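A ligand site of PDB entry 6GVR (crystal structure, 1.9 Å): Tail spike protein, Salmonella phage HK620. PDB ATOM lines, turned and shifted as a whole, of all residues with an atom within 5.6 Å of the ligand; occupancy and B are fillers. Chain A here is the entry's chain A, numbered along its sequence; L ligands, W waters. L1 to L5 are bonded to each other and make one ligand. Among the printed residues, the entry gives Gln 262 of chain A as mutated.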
ATOM      1  N   GLY A 101     -18.964  15.228 -17.039  1.00  0.00           N
ATOM      2  CA  GLY A 101     -17.993  15.071 -18.124  1.00  0.00           C
ATOM      3  C   GLY A 101     -16.573  14.748 -17.664  1.00  0.00           C
ATOM      4  O   GLY A 101     -15.723  14.381 -18.486  1.00  0.00           O
ATOM      5  N   HIS A 102     -16.289  14.895 -16.357  1.00  0.00           N
ATOM      6  CA  HIS A 102     -15.043  14.525 -15.774  1.00  0.00           C
ATOM      7  C   HIS A 102     -15.165  13.256 -14.952  1.00  0.00           C
ATOM      8  O   HIS A 102     -14.266  12.978 -14.102  1.00  0.00           O
ATOM      9  CB  HIS A 102     -14.550  15.647 -14.848  1.00  0.00           C
ATOM     10  CG  HIS A 102     -14.480  16.971 -15.481  1.00  0.00           C
ATOM     11  ND1 HIS A 102     -13.339  17.472 -16.058  1.00  0.00           N
ATOM     12  CD2 HIS A 102     -15.403  17.952 -15.584  1.00  0.00           C
ATOM     13  CE1 HIS A 102     -13.552  18.680 -16.515  1.00  0.00           C
ATOM     14  NE2 HIS A 102     -14.814  19.000 -16.238  1.00  0.00           N
ATOM     15  N   SER A 103     -16.254  12.491 -15.149  1.00  0.00           N
ATOM     16  CA  SER A 103     -16.598  11.304 -14.307  1.00  0.00           C
ATOM     17  C   SER A 103     -16.580  11.656 -12.822  1.00  0.00           C
ATOM     18  O   SER A 103     -16.183  10.804 -11.999  1.00  0.00           O
ATOM     19  CB  SER A 103     -15.594  10.159 -14.580  1.00  0.00           C
ATOM     20  OG  SER A 103     -15.685   9.816 -15.941  1.00  0.00           O
ATOM     21  N   GLN A 132     -13.400  10.504 -10.731  1.00  0.00           N
ATOM     22  CA  GLN A 132     -12.596  11.597 -10.169  1.00  0.00           C
ATOM     23  C   GLN A 132     -13.342  12.047  -8.933  1.00  0.00           C
ATOM     24  O   GLN A 132     -14.465  12.497  -9.016  1.00  0.00           O
ATOM     25  CB  GLN A 132     -12.388  12.712 -11.199  1.00  0.00           C
ATOM     26  CG  GLN A 132     -11.487  12.288 -12.370  1.00  0.00           C
ATOM     27  CD  GLN A 132     -11.010  13.491 -13.169  1.00  0.00           C
ATOM     28  OE1 GLN A 132     -10.258  14.353 -12.661  1.00  0.00           O
ATOM     29  NE2 GLN A 132     -11.383  13.545 -14.462  1.00  0.00           N
ATOM     30  N   PHE A 137     -13.867  21.661 -11.334  1.00  0.00           N
ATOM     31  CA  PHE A 137     -14.455  22.268 -12.538  1.00  0.00           C
ATOM     32  C   PHE A 137     -15.940  22.375 -12.325  1.00  0.00           C
ATOM     33  O   PHE A 137     -16.537  21.591 -11.558  1.00  0.00           O
ATOM     34  CB  PHE A 137     -14.168  21.502 -13.817  1.00  0.00           C
ATOM     35  CG  PHE A 137     -12.680  21.329 -14.157  1.00  0.00           C
ATOM     36  CD1 PHE A 137     -11.930  22.352 -14.710  1.00  0.00           C
ATOM     37  CD2 PHE A 137     -12.069  20.114 -13.935  1.00  0.00           C
ATOM     38  CE1 PHE A 137     -10.592  22.116 -15.062  1.00  0.00           C
ATOM     39  CE2 PHE A 137     -10.760  19.864 -14.276  1.00  0.00           C
ATOM     40  CZ  PHE A 137     -10.039  20.845 -14.863  1.00  0.00           C
ATOM     41  N   PRO A 142     -13.366  22.215 -19.682  1.00  0.00           N
ATOM     42  CA  PRO A 142     -12.557  23.092 -18.808  1.00  0.00           C
ATOM     43  C   PRO A 142     -12.309  24.514 -19.307  1.00  0.00           C
ATOM     44  O   PRO A 142     -12.228  25.495 -18.515  1.00  0.00           O
ATOM     45  CB  PRO A 142     -11.254  22.302 -18.594  1.00  0.00           C
ATOM     46  CG  PRO A 142     -11.403  20.988 -19.286  1.00  0.00           C
ATOM     47  CD  PRO A 142     -12.759  20.893 -19.919  1.00  0.00           C
ATOM     48  N   LEU A 172      -9.644   7.138 -17.080  1.00  0.00           N
ATOM     49  CA  LEU A 172      -8.923   8.001 -16.110  1.00  0.00           C
ATOM     50  C   LEU A 172      -9.544   7.884 -14.732  1.00  0.00           C
ATOM     51  O   LEU A 172     -10.770   7.716 -14.572  1.00  0.00           O
ATOM     52  CB  LEU A 172      -8.947   9.443 -16.530  1.00  0.00           C
ATOM     53  CG  LEU A 172      -8.375   9.722 -17.900  1.00  0.00           C
ATOM     54  CD1 LEU A 172      -8.810  11.135 -18.295  1.00  0.00           C
ATOM     55  CD2 LEU A 172      -6.868   9.501 -17.996  1.00  0.00           C
ATOM     56  N   ASN A 174      -8.918   9.813 -10.733  1.00  0.00           N
ATOM     57  CA  ASN A 174      -8.291  10.904  -9.918  1.00  0.00           C
ATOM     58  C   ASN A 174      -8.914  10.882  -8.503  1.00  0.00           C
ATOM     59  O   ASN A 174     -10.067  10.520  -8.299  1.00  0.00           O
ATOM     60  CB  ASN A 174      -8.493  12.281 -10.633  1.00  0.00           C
ATOM     61  CG  ASN A 174      -7.523  13.377 -10.143  1.00  0.00           C
ATOM     62  OD1 ASN A 174      -6.670  13.147  -9.252  1.00  0.00           O
ATOM     63  ND2 ASN A 174      -7.616  14.589 -10.744  1.00  0.00           N
ATOM     64  N   THR A 197      -4.937   7.176 -12.081  1.00  0.00           N
ATOM     65  CA  THR A 197      -4.058   7.864 -12.997  1.00  0.00           C
ATOM     66  C   THR A 197      -3.273   8.921 -12.154  1.00  0.00           C
ATOM     67  O   THR A 197      -2.066   9.065 -12.285  1.00  0.00           O
ATOM     68  CB  THR A 197      -4.845   8.587 -14.042  1.00  0.00           C
ATOM     69  OG1 THR A 197      -5.724   7.666 -14.740  1.00  0.00           O
ATOM     70  CG2 THR A 197      -3.946   9.273 -15.007  1.00  0.00           C
ATOM     71  N   TRP A 198      -4.007   9.601 -11.332  1.00  0.00           N
ATOM     72  CA  TRP A 198      -3.485  10.598 -10.365  1.00  0.00           C
ATOM     73  C   TRP A 198      -4.218  10.514  -9.037  1.00  0.00           C
ATOM     74  O   TRP A 198      -5.354  10.008  -8.975  1.00  0.00           O
ATOM     75  CB  TRP A 198      -3.689  12.005 -10.857  1.00  0.00           C
ATOM     76  CG  TRP A 198      -3.362  12.300 -12.321  1.00  0.00           C
ATOM     77  CD1 TRP A 198      -2.146  12.440 -12.889  1.00  0.00           C
ATOM     78  CD2 TRP A 198      -4.325  12.424 -13.387  1.00  0.00           C
ATOM     79  NE1 TRP A 198      -2.271  12.708 -14.227  1.00  0.00           N
ATOM     80  CE2 TRP A 198      -3.622  12.709 -14.556  1.00  0.00           C
ATOM     81  CE3 TRP A 198      -5.728  12.392 -13.433  1.00  0.00           C
ATOM     82  CZ2 TRP A 198      -4.251  12.903 -15.761  1.00  0.00           C
ATOM     83  CZ3 TRP A 198      -6.358  12.521 -14.684  1.00  0.00           C
ATOM     84  CH2 TRP A 198      -5.618  12.823 -15.803  1.00  0.00           C
ATOM     85  N   THR A 201      -4.647  16.588  -8.855  1.00  0.00           N
ATOM     86  CA  THR A 201      -4.166  17.465  -9.907  1.00  0.00           C
ATOM     87  C   THR A 201      -4.476  18.889  -9.545  1.00  0.00           C
ATOM     88  O   THR A 201      -5.541  19.145  -8.977  1.00  0.00           O
ATOM     89  CB  THR A 201      -4.832  17.179 -11.241  1.00  0.00           C
ATOM     90  OG1 THR A 201      -6.238  17.427 -11.189  1.00  0.00           O
ATOM     91  CG2 THR A 201      -4.595  15.757 -11.663  1.00  0.00           C
ATOM     92  N   LEU A 202      -3.575  19.802  -9.897  1.00  0.00           N
ATOM     93  CA  LEU A 202      -3.657  21.196  -9.476  1.00  0.00           C
ATOM     94  C   LEU A 202      -3.668  22.030 -10.738  1.00  0.00           C
ATOM     95  O   LEU A 202      -2.874  21.831 -11.634  1.00  0.00           O
ATOM     96  CB  LEU A 202      -2.492  21.612  -8.629  1.00  0.00           C
ATOM     97  CG  LEU A 202      -2.116  20.776  -7.441  1.00  0.00           C
ATOM     98  CD1 LEU A 202      -0.895  21.466  -6.764  1.00  0.00           C
ATOM     99  CD2 LEU A 202      -3.255  20.538  -6.483  1.00  0.00           C
ATOM    100  N   GLY A 203      -4.592  22.939 -10.839  1.00  0.00           N
ATOM    101  CA  GLY A 203      -4.608  23.772 -12.043  1.00  0.00           C
ATOM    102  C   GLY A 203      -5.161  23.052 -13.289  1.00  0.00           C
ATOM    103  O   GLY A 203      -5.478  21.804 -13.255  1.00  0.00           O
ATOM    104  N   TRP A 204      -5.273  23.827 -14.346  1.00  0.00           N
ATOM    105  CA  TRP A 204      -5.665  23.304 -15.701  1.00  0.00           C
ATOM    106  C   TRP A 204      -4.965  24.146 -16.714  1.00  0.00           C
ATOM    107  O   TRP A 204      -5.273  25.364 -16.819  1.00  0.00           O
ATOM    108  CB  TRP A 204      -7.176  23.288 -15.924  1.00  0.00           C
ATOM    109  CG  TRP A 204      -7.495  22.871 -17.317  1.00  0.00           C
ATOM    110  CD1 TRP A 204      -7.346  21.631 -17.835  1.00  0.00           C
ATOM    111  CD2 TRP A 204      -7.876  23.731 -18.426  1.00  0.00           C
ATOM    112  NE1 TRP A 204      -7.676  21.619 -19.195  1.00  0.00           N
ATOM    113  CE2 TRP A 204      -7.968  22.903 -19.589  1.00  0.00           C
ATOM    114  CE3 TRP A 204      -8.157  25.079 -18.549  1.00  0.00           C
ATOM    115  CZ2 TRP A 204      -8.316  23.391 -20.823  1.00  0.00           C
ATOM    116  CZ3 TRP A 204      -8.500  25.586 -19.773  1.00  0.00           C
ATOM    117  CH2 TRP A 204      -8.605  24.721 -20.914  1.00  0.00           C
ATOM    118  N   ASN A 205      -4.046  23.522 -17.455  1.00  0.00           N
ATOM    119  CA  ASN A 205      -3.301  24.169 -18.529  1.00  0.00           C
ATOM    120  C   ASN A 205      -2.851  25.581 -18.226  1.00  0.00           C
ATOM    121  O   ASN A 205      -3.020  26.532 -18.996  1.00  0.00           O
ATOM    122  CB  ASN A 205      -4.086  24.074 -19.815  1.00  0.00           C
ATOM    123  CG  ASN A 205      -4.232  22.650 -20.315  1.00  0.00           C
ATOM    124  OD1 ASN A 205      -3.782  21.650 -19.676  1.00  0.00           O
ATOM    125  ND2 ASN A 205      -5.030  22.521 -21.377  1.00  0.00           N
ATOM    126  N   ASP A 229      -0.780   4.452 -16.968  1.00  0.00           N
ATOM    127  CA  ASP A 229       0.170   5.510 -16.588  1.00  0.00           C
ATOM    128  C   ASP A 229      -0.279   6.130 -15.293  1.00  0.00           C
ATOM    129  O   ASP A 229      -1.503   6.272 -15.047  1.00  0.00           O
ATOM    130  CB  ASP A 229       0.186   6.575 -17.687  1.00  0.00           C
ATOM    131  CG  ASP A 229       1.383   7.463 -17.614  1.00  0.00           C
ATOM    132  OD1 ASP A 229       2.301   7.337 -16.686  1.00  0.00           O
ATOM    133  OD2 ASP A 229       1.362   8.305 -18.509  1.00  0.00           O
ATOM    134  N   HIS A 230       0.659   6.512 -14.455  1.00  0.00           N
ATOM    135  CA  HIS A 230       0.312   7.122 -13.203  1.00  0.00           C
ATOM    136  C   HIS A 230       1.314   8.227 -12.830  1.00  0.00           C
ATOM    137  O   HIS A 230       2.504   8.052 -12.939  1.00  0.00           O
ATOM    138  CB  HIS A 230       0.262   6.111 -12.060  1.00  0.00           C
ATOM    139  CG  HIS A 230       0.084   6.734 -10.712  1.00  0.00           C
ATOM    140  ND1 HIS A 230      -1.135   6.742 -10.040  1.00  0.00           N
ATOM    141  CD2 HIS A 230       0.986   7.315  -9.887  1.00  0.00           C
ATOM    142  CE1 HIS A 230      -0.945   7.345  -8.874  1.00  0.00           C
ATOM    143  NE2 HIS A 230       0.328   7.695  -8.763  1.00  0.00           N
ATOM    144  N   SER A 231       0.754   9.355 -12.400  1.00  0.00           N
ATOM    145  CA  SER A 231       1.563  10.460 -11.782  1.00  0.00           C
ATOM    146  C   SER A 231       0.785  10.901 -10.564  1.00  0.00           C
ATOM    147  O   SER A 231      -0.375  11.331 -10.722  1.00  0.00           O
ATOM    148  CB  SER A 231       1.767  11.623 -12.753  1.00  0.00           C
ATOM    149  OG  SER A 231       2.645  11.212 -13.813  1.00  0.00           O
ATOM    150  N   TYR A 234      -0.101  16.104 -10.148  1.00  0.00           N
ATOM    151  CA  TYR A 234       0.176  16.803 -11.409  1.00  0.00           C
ATOM    152  C   TYR A 234      -0.028  18.291 -11.149  1.00  0.00           C
ATOM    153  O   TYR A 234      -1.142  18.755 -10.826  1.00  0.00           O
ATOM    154  CB  TYR A 234      -0.792  16.358 -12.510  1.00  0.00           C
ATOM    155  CG  TYR A 234      -0.394  16.572 -13.960  1.00  0.00           C
ATOM    156  CD1 TYR A 234      -0.366  17.845 -14.520  1.00  0.00           C
ATOM    157  CD2 TYR A 234      -0.081  15.498 -14.811  1.00  0.00           C
ATOM    158  CE1 TYR A 234      -0.027  18.026 -15.861  1.00  0.00           C
ATOM    159  CE2 TYR A 234       0.240  15.680 -16.143  1.00  0.00           C
ATOM    160  CZ  TYR A 234       0.204  16.951 -16.696  1.00  0.00           C
ATOM    161  OH  TYR A 234       0.478  17.116 -18.033  1.00  0.00           O
ATOM    162  N   ASN A 236      -0.244  21.768 -12.537  1.00  0.00           N
ATOM    163  CA  ASN A 236      -0.518  22.420 -13.852  1.00  0.00           C
ATOM    164  C   ASN A 236      -1.012  23.861 -13.709  1.00  0.00           C
ATOM    165  O   ASN A 236      -1.661  24.464 -14.581  1.00  0.00           O
ATOM    166  CB  ASN A 236      -1.488  21.582 -14.649  1.00  0.00           C
ATOM    167  CG  ASN A 236      -1.331  21.728 -16.157  1.00  0.00           C
ATOM    168  OD1 ASN A 236      -0.414  22.374 -16.651  1.00  0.00           O
ATOM    169  ND2 ASN A 236      -2.321  21.126 -16.935  1.00  0.00           N
ATOM    170  N   GLN A 262       4.429  15.709 -11.271  1.00  0.00           N
ATOM    171  CA  GLN A 262       4.606  16.414 -12.554  1.00  0.00           C
ATOM    172  C   GLN A 262       4.708  17.915 -12.240  1.00  0.00           C
ATOM    173  O   GLN A 262       3.723  18.429 -11.722  1.00  0.00           O
ATOM    174  CB  GLN A 262       3.385  16.173 -13.522  1.00  0.00           C
ATOM    175  CG  GLN A 262       3.189  14.683 -13.893  1.00  0.00           C
ATOM    176  CD  GLN A 262       4.187  14.091 -14.928  1.00  0.00           C
ATOM    177  OE1 GLN A 262       4.472  12.861 -14.871  1.00  0.00           O
ATOM    178  NE2 GLN A 262       4.666  14.889 -15.891  1.00  0.00           N
ATOM    179  N   HIS A 264       4.651  21.268 -14.209  1.00  0.00           N
ATOM    180  CA  HIS A 264       4.389  21.608 -15.603  1.00  0.00           C
ATOM    181  C   HIS A 264       4.122  23.058 -15.839  1.00  0.00           C
ATOM    182  O   HIS A 264       3.707  23.394 -16.975  1.00  0.00           O
ATOM    183  CB  HIS A 264       3.231  20.812 -16.148  1.00  0.00           C
ATOM    184  CG  HIS A 264       3.585  19.441 -16.560  1.00  0.00           C
ATOM    185  ND1 HIS A 264       3.058  18.851 -17.688  1.00  0.00           N
ATOM    186  CD2 HIS A 264       4.454  18.544 -16.046  1.00  0.00           C
ATOM    187  CE1 HIS A 264       3.558  17.632 -17.828  1.00  0.00           C
ATOM    188  NE2 HIS A 264       4.348  17.389 -16.815  1.00  0.00           N
ATOM    189  N   TYR A 283       8.726  14.596 -13.395  1.00  0.00           N
ATOM    190  CA  TYR A 283       8.917  15.223 -14.693  1.00  0.00           C
ATOM    191  C   TYR A 283       8.870  16.750 -14.501  1.00  0.00           C
ATOM    192  O   TYR A 283       8.030  17.243 -13.754  1.00  0.00           O
ATOM    193  CB  TYR A 283       7.825  14.848 -15.663  1.00  0.00           C
ATOM    194  CG  TYR A 283       7.900  13.443 -16.235  1.00  0.00           C
ATOM    195  CD1 TYR A 283       7.384  12.357 -15.521  1.00  0.00           C
ATOM    196  CD2 TYR A 283       8.433  13.210 -17.531  1.00  0.00           C
ATOM    197  CE1 TYR A 283       7.347  11.050 -16.098  1.00  0.00           C
ATOM    198  CE2 TYR A 283       8.464  11.882 -18.058  1.00  0.00           C
ATOM    199  CZ  TYR A 283       7.933  10.824 -17.331  1.00  0.00           C
ATOM    200  OH  TYR A 283       7.941   9.545 -17.884  1.00  0.00           O
ATOM    201  N   VAL A 285       8.581  19.725 -17.026  1.00  0.00           N
ATOM    202  CA  VAL A 285       8.252  19.706 -18.476  1.00  0.00           C
ATOM    203  C   VAL A 285       7.409  20.918 -18.811  1.00  0.00           C
ATOM    204  O   VAL A 285       6.433  21.154 -18.082  1.00  0.00           O
ATOM    205  CB  VAL A 285       7.433  18.431 -18.877  1.00  0.00           C
ATOM    206  CG1 VAL A 285       6.869  18.547 -20.313  1.00  0.00           C
ATOM    207  CG2 VAL A 285       8.277  17.183 -18.814  1.00  0.00           C
ATOM    208  N   HIS A 287       4.822  21.590 -21.631  1.00  0.00           N
ATOM    209  CA  HIS A 287       4.083  21.078 -22.808  1.00  0.00           C
ATOM    210  C   HIS A 287       3.438  22.309 -23.514  1.00  0.00           C
ATOM    211  O   HIS A 287       2.593  22.981 -22.943  1.00  0.00           O
ATOM    212  CB  HIS A 287       2.956  20.137 -22.416  1.00  0.00           C
ATOM    213  CG  HIS A 287       3.342  18.727 -22.053  1.00  0.00           C
ATOM    214  ND1 HIS A 287       4.181  17.956 -22.816  1.00  0.00           N
ATOM    215  CD2 HIS A 287       2.798  17.884 -21.131  1.00  0.00           C
ATOM    216  CE1 HIS A 287       4.257  16.737 -22.296  1.00  0.00           C
ATOM    217  NE2 HIS A 287       3.454  16.676 -21.249  1.00  0.00           N
ATOM    218  N   ALA A 289       1.022  22.275 -25.387  1.00  0.00           N
ATOM    219  CA  ALA A 289      -0.393  22.077 -25.246  1.00  0.00           C
ATOM    220  C   ALA A 289      -1.032  22.536 -23.948  1.00  0.00           C
ATOM    221  O   ALA A 289      -2.267  22.647 -23.863  1.00  0.00           O
ATOM    222  CB  ALA A 289      -0.747  20.618 -25.533  1.00  0.00           C
ATOM    223  N   GLU A 290      -0.241  22.853 -22.932  1.00  0.00           N
ATOM    224  CA  GLU A 290      -0.739  23.237 -21.662  1.00  0.00           C
ATOM    225  C   GLU A 290      -0.399  24.667 -21.357  1.00  0.00           C
ATOM    226  O   GLU A 290      -0.374  25.096 -20.179  1.00  0.00           O
ATOM    227  CB  GLU A 290      -0.074  22.309 -20.560  1.00  0.00           C
ATOM    228  CG  GLU A 290      -0.474  20.847 -20.714  1.00  0.00           C
ATOM    229  CD  GLU A 290       0.095  19.966 -19.628  1.00  0.00           C
ATOM    230  OE1 GLU A 290       1.241  20.282 -19.183  1.00  0.00           O
ATOM    231  OE2 GLU A 290      -0.574  18.970 -19.301  1.00  0.00           O
ATOM    232  N   PRO A 359      10.966  14.453 -23.015  1.00  0.00           N
ATOM    233  CA  PRO A 359      10.270  13.226 -22.482  1.00  0.00           C
ATOM    234  C   PRO A 359       9.830  12.249 -23.668  1.00  0.00           C
ATOM    235  O   PRO A 359      10.294  11.089 -23.795  1.00  0.00           O
ATOM    236  CB  PRO A 359       9.028  13.841 -21.764  1.00  0.00           C
ATOM    237  CG  PRO A 359       8.765  15.208 -22.467  1.00  0.00           C
ATOM    238  CD  PRO A 359       9.948  15.482 -23.406  1.00  0.00           C
HETATM  239  C1  LIG L   1       3.671  11.568 -17.656  1.00  0.00           C
HETATM  240  C2  LIG L   1       2.228  12.109 -17.757  1.00  0.00           C
HETATM  241  C3  LIG L   1       1.946  12.595 -19.199  1.00  0.00           C
HETATM  242  C4  LIG L   1       3.020  13.620 -19.588  1.00  0.00           C
HETATM  243  C5  LIG L   1       4.434  13.021 -19.428  1.00  0.00           C
HETATM  244  C6  LIG L   1       5.565  13.974 -19.629  1.00  0.00           C
HETATM  245  C7  LIG L   1       0.391  11.256 -16.316  1.00  0.00           C
HETATM  246  C8  LIG L   1      -0.375  10.055 -15.904  1.00  0.00           C
HETATM  247  O1  LIG L   1       4.620  12.536 -18.116  1.00  0.00           O
HETATM  248  O2  LIG L   1       0.634  13.248 -19.221  1.00  0.00           O
HETATM  249  O3  LIG L   1       2.848  14.196 -20.897  1.00  0.00           O
HETATM  250  O4  LIG L   1       5.412  14.916 -18.539  1.00  0.00           O
HETATM  251  O5  LIG L   1       0.154  12.364 -15.814  1.00  0.00           O
HETATM  252  N1  LIG L   1       1.313  11.079 -17.294  1.00  0.00           N
HETATM  253  O6  LIG L   1       3.820  10.465 -18.497  1.00  0.00           O
HETATM  254  C1  LG2 L   2      -0.072  13.109 -20.457  1.00  0.00           C
HETATM  255  C2  LG2 L   2      -1.051  14.258 -20.499  1.00  0.00           C
HETATM  256  C3  LG2 L   2      -2.126  14.170 -19.390  1.00  0.00           C
HETATM  257  C4  LG2 L   2      -2.741  12.769 -19.347  1.00  0.00           C
HETATM  258  C5  LG2 L   2      -1.629  11.705 -19.288  1.00  0.00           C
HETATM  259  C6  LG2 L   2      -2.090  10.257 -19.314  1.00  0.00           C
HETATM  260  O1  LG2 L   2      -0.331  15.507 -20.368  1.00  0.00           O
HETATM  261  O2  LG2 L   2      -3.098  15.186 -19.686  1.00  0.00           O
HETATM  262  O3  LG2 L   2      -3.514  12.553 -20.559  1.00  0.00           O
HETATM  263  O4  LG2 L   2      -0.715  11.900 -20.386  1.00  0.00           O
HETATM  264  O5  LG2 L   2      -3.028  10.085 -18.265  1.00  0.00           O
HETATM  265  C1  LG3 L   3      -4.833  12.011 -20.256  1.00  0.00           C
HETATM  266  C2  LG3 L   3      -5.514  11.551 -21.569  1.00  0.00           C
HETATM  267  C3  LG3 L   3      -5.760  12.701 -22.549  1.00  0.00           C
HETATM  268  C4  LG3 L   3      -6.596  13.677 -21.809  1.00  0.00           C
HETATM  269  C5  LG3 L   3      -5.888  14.133 -20.532  1.00  0.00           C
HETATM  270  C6  LG3 L   3      -6.692  15.168 -19.731  1.00  0.00           C
HETATM  271  O1  LG3 L   3      -4.738  10.604 -22.179  1.00  0.00           O
HETATM  272  O2  LG3 L   3      -6.536  12.197 -23.619  1.00  0.00           O
HETATM  273  O3  LG3 L   3      -6.921  14.730 -22.674  1.00  0.00           O
HETATM  274  O4  LG3 L   3      -5.662  12.981 -19.663  1.00  0.00           O
HETATM  275  O5  LG3 L   3      -7.991  14.654 -19.296  1.00  0.00           O
HETATM  276  C1  LG4 L   4      -3.089  16.240 -18.723  1.00  0.00           C
HETATM  277  C2  LG4 L   4      -3.761  17.453 -19.347  1.00  0.00           C
HETATM  278  C3  LG4 L   4      -3.916  18.598 -18.359  1.00  0.00           C
HETATM  279  C4  LG4 L   4      -4.431  18.155 -17.026  1.00  0.00           C
HETATM  280  C5  LG4 L   4      -3.580  17.012 -16.586  1.00  0.00           C
HETATM  281  C6  LG4 L   4      -3.935  16.587 -15.199  1.00  0.00           C
HETATM  282  C7  LG4 L   4      -3.429  17.863 -21.716  1.00  0.00           C
HETATM  283  C8  LG4 L   4      -2.491  18.255 -22.841  1.00  0.00           C
HETATM  284  N1  LG4 L   4      -2.953  17.849 -20.464  1.00  0.00           N
HETATM  285  O1  LG4 L   4      -4.841  19.462 -18.940  1.00  0.00           O
HETATM  286  O2  LG4 L   4      -4.235  19.243 -16.115  1.00  0.00           O
HETATM  287  O3  LG4 L   4      -3.730  15.890 -17.494  1.00  0.00           O
HETATM  288  O4  LG4 L   4      -5.218  16.049 -15.256  1.00  0.00           O
HETATM  289  O5  LG4 L   4      -4.604  17.645 -21.951  1.00  0.00           O
HETATM  290  C1  LG5 L   5      -9.062  15.438 -19.879  1.00  0.00           C
HETATM  291  C2  LG5 L   5     -10.367  14.670 -19.652  1.00  0.00           C
HETATM  292  C3  LG5 L   5     -10.776  14.633 -18.184  1.00  0.00           C
HETATM  293  C4  LG5 L   5     -10.703  16.059 -17.607  1.00  0.00           C
HETATM  294  C5  LG5 L   5      -9.377  16.760 -17.970  1.00  0.00           C
HETATM  295  C6  LG5 L   5      -9.294  18.236 -17.532  1.00  0.00           C
HETATM  296  O1  LG5 L   5     -11.302  15.368 -20.455  1.00  0.00           O
HETATM  297  O2  LG5 L   5     -12.086  14.016 -18.044  1.00  0.00           O
HETATM  298  O3  LG5 L   5     -10.985  15.998 -16.197  1.00  0.00           O
HETATM  299  O4  LG5 L   5      -9.143  16.769 -19.384  1.00  0.00           O
HETATM  300  O   HOH W   1      -3.576   7.420 -18.450  1.00  0.00           O
HETATM  301  O   HOH W   2       0.375  15.897 -23.018  1.00  0.00           O
HETATM  302  O   HOH W   3       5.309   8.370 -17.969  1.00  0.00           O
HETATM  303  O   HOH W   4      -7.189  17.494 -13.806  1.00  0.00           O
HETATM  304  O   HOH W   5     -13.909  16.972 -19.583  1.00  0.00           O
HETATM  305  O   HOH W   6     -12.641  11.362 -16.850  1.00  0.00           O
HETATM  306  O   HOH W   7     -10.396  15.041 -22.965  1.00  0.00           O
HETATM  307  O   HOH W   8      -9.708  16.438 -13.890  1.00  0.00           O
HETATM  308  O   HOH W   9      -5.951  20.006 -22.469  1.00  0.00           O
HETATM  309  O   HOH W  10      -6.618  19.866 -14.954  1.00  0.00           O
HETATM  310  O   HOH W  11       3.103  12.863 -23.066  1.00  0.00           O
HETATM  311  O   HOH W  12      -6.098   8.395 -21.902  1.00  0.00           O
HETATM  312  O   HOH W  13      -2.146  11.609 -23.084  1.00  0.00           O
HETATM  313  O   HOH W  14     -13.515  12.844 -19.997  1.00  0.00           O
HETATM  314  O   HOH W  15      -7.324  18.891 -20.340  1.00  0.00           O
HETATM  315  O   HOH W  16      -6.942  13.716 -25.875  1.00  0.00           O
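Water W3 lies within hydrogen-bond range of O6 of LIG L1, OH of Tyr 283 and OD1 of Asp 229. Water W10 bridges an oxygen (O2) of LG4 L4 (2.7 Å) and the backbone carbonyl oxygen of Gly 203 (2.8 Å). Water W4 lies within hydrogen-bond range of the side-chain hydroxyl (OG1) of Thr 201 (2.8 Å) and an oxygen (O4) of LG4 L4 (2.8 Å). Water W15 lies within hydrogen-bond range of O1 of LG4 L4 and NE1 of Trp 204. Water W6 lies within hydrogen-bond range of O2 of LG5 L5 (3.0 Å) and NE2 of Gln 132 (3.5 Å). Water W5 bridges an oxygen (O1) of LG5 L5 (3.2 Å) and the backbone carbonyl oxygen of Gly 101 (3.3 Å).
Merely in contact with the ligand: Gly 101 (3.7 Å), Phe 137 (3.8 Å), Pro 142 (3.9 Å), Leu 172 (3.7 Å), Thr 197 (3.5 Å), Thr 201 (3.7 Å), Trp 204 (3.5 Å), His 230 (3.96 Å), Tyr 283 (3.6 Å), Val 285 (3.7 Å) and Ala 289 (3.98 Å). Hydrophobic or aromatic side chains within 4 Å of the ligand: His 102, Phe 137, Pro 142, Leu 172, Trp 198, Trp 204, Tyr 234, His 264, Tyr 283, Val 285, His 287 and Ala 289. Within 4 Å of the ligand: Gly 101, His 102, Gln 132, Phe 137, Pro 142, Leu 172, Thr 197, Trp 198, Thr 201, Trp 204, Asn 205, Asp 229, His 230, Ser 231, Tyr 234, Asn 236, Gln 262, His 264, Tyr 283, Val 285, His 287, Ala 289 and Glu 290. The nearest printed residue that does not touch the ligand is Gly 203 (4.04 Å).
The side-chain amide oxygen (OD1) of Asn 205 sits at hydrogen-bond distance from an oxygen (O1) of LG4 L4 (2.5 Å). NE2 of His 287 is in hydrogen-bond range of O3 of LIG L1. The side-chain amide nitrogen of Gln 262 is in hydrogen-bond range of an oxygen (O4) of LIG L1. A ring nitrogen (ND1) of His 102 sits at hydrogen-bond distance from an oxygen (O3) of LG5 L5, 2.8 Å away. An oxygen (O2) of LG4 L4 lies within hydrogen-bond range of the side-chain amide nitrogen (ND2) of Asn 236. The side-chain carboxylate (OE2) of Glu 290 is in hydrogen-bond range of a nitrogen (N1) of LG4 L4, at 2.9 Å. The indole nitrogen (NE1) of Trp 198 sits at hydrogen-bond distance from an oxygen (O5) of LIG L1, 2.9 Å away. OH of Tyr 234 sits at hydrogen-bond distance from O1 of LG2 L2 (2.9 Å). The side-chain carboxylate of Asp 229 sits at hydrogen-bond distance from a nitrogen (N1) of LIG L1 (3.0 Å). An oxygen (O3) of LG5 L5 lies within hydrogen-bond range of the side-chain amide nitrogen (NE2) of Gln 132 (3.0 Å). A ring nitrogen (NE2) of His 264 lies within hydrogen-bond range of an oxygen (O4) of LIG L1 (3.2 Å). OG of Ser 231 sits close to O5 of LIG L1 (3.4 Å).
N of Asn 205 lies close to ND2 of Asn 236 (3.0 Å). N of Asn 236 is in hydrogen-bond range of O of Leu 202 (2.8 Å). O of Trp 198 lies close to OD1 of Asn 174. OH of Tyr 234 lies within hydrogen-bond range of ND1 of His 264 (3.1 Å). The side-chain amide nitrogen of Asn 174 lies within hydrogen-bond range of the side-chain amide oxygen of Gln 132 (3.3 Å). The backbone NH (N) of Ser 231 sits at hydrogen-bond distance from the backbone carbonyl oxygen (O) of Thr 197 (2.8 Å). A ring nitrogen (ND1) of His 230 lies close to the backbone carbonyl oxygen of Thr 197 (3.4 Å). OG1 of Thr 201 lies within hydrogen-bond range of ND2 of Asn 174.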
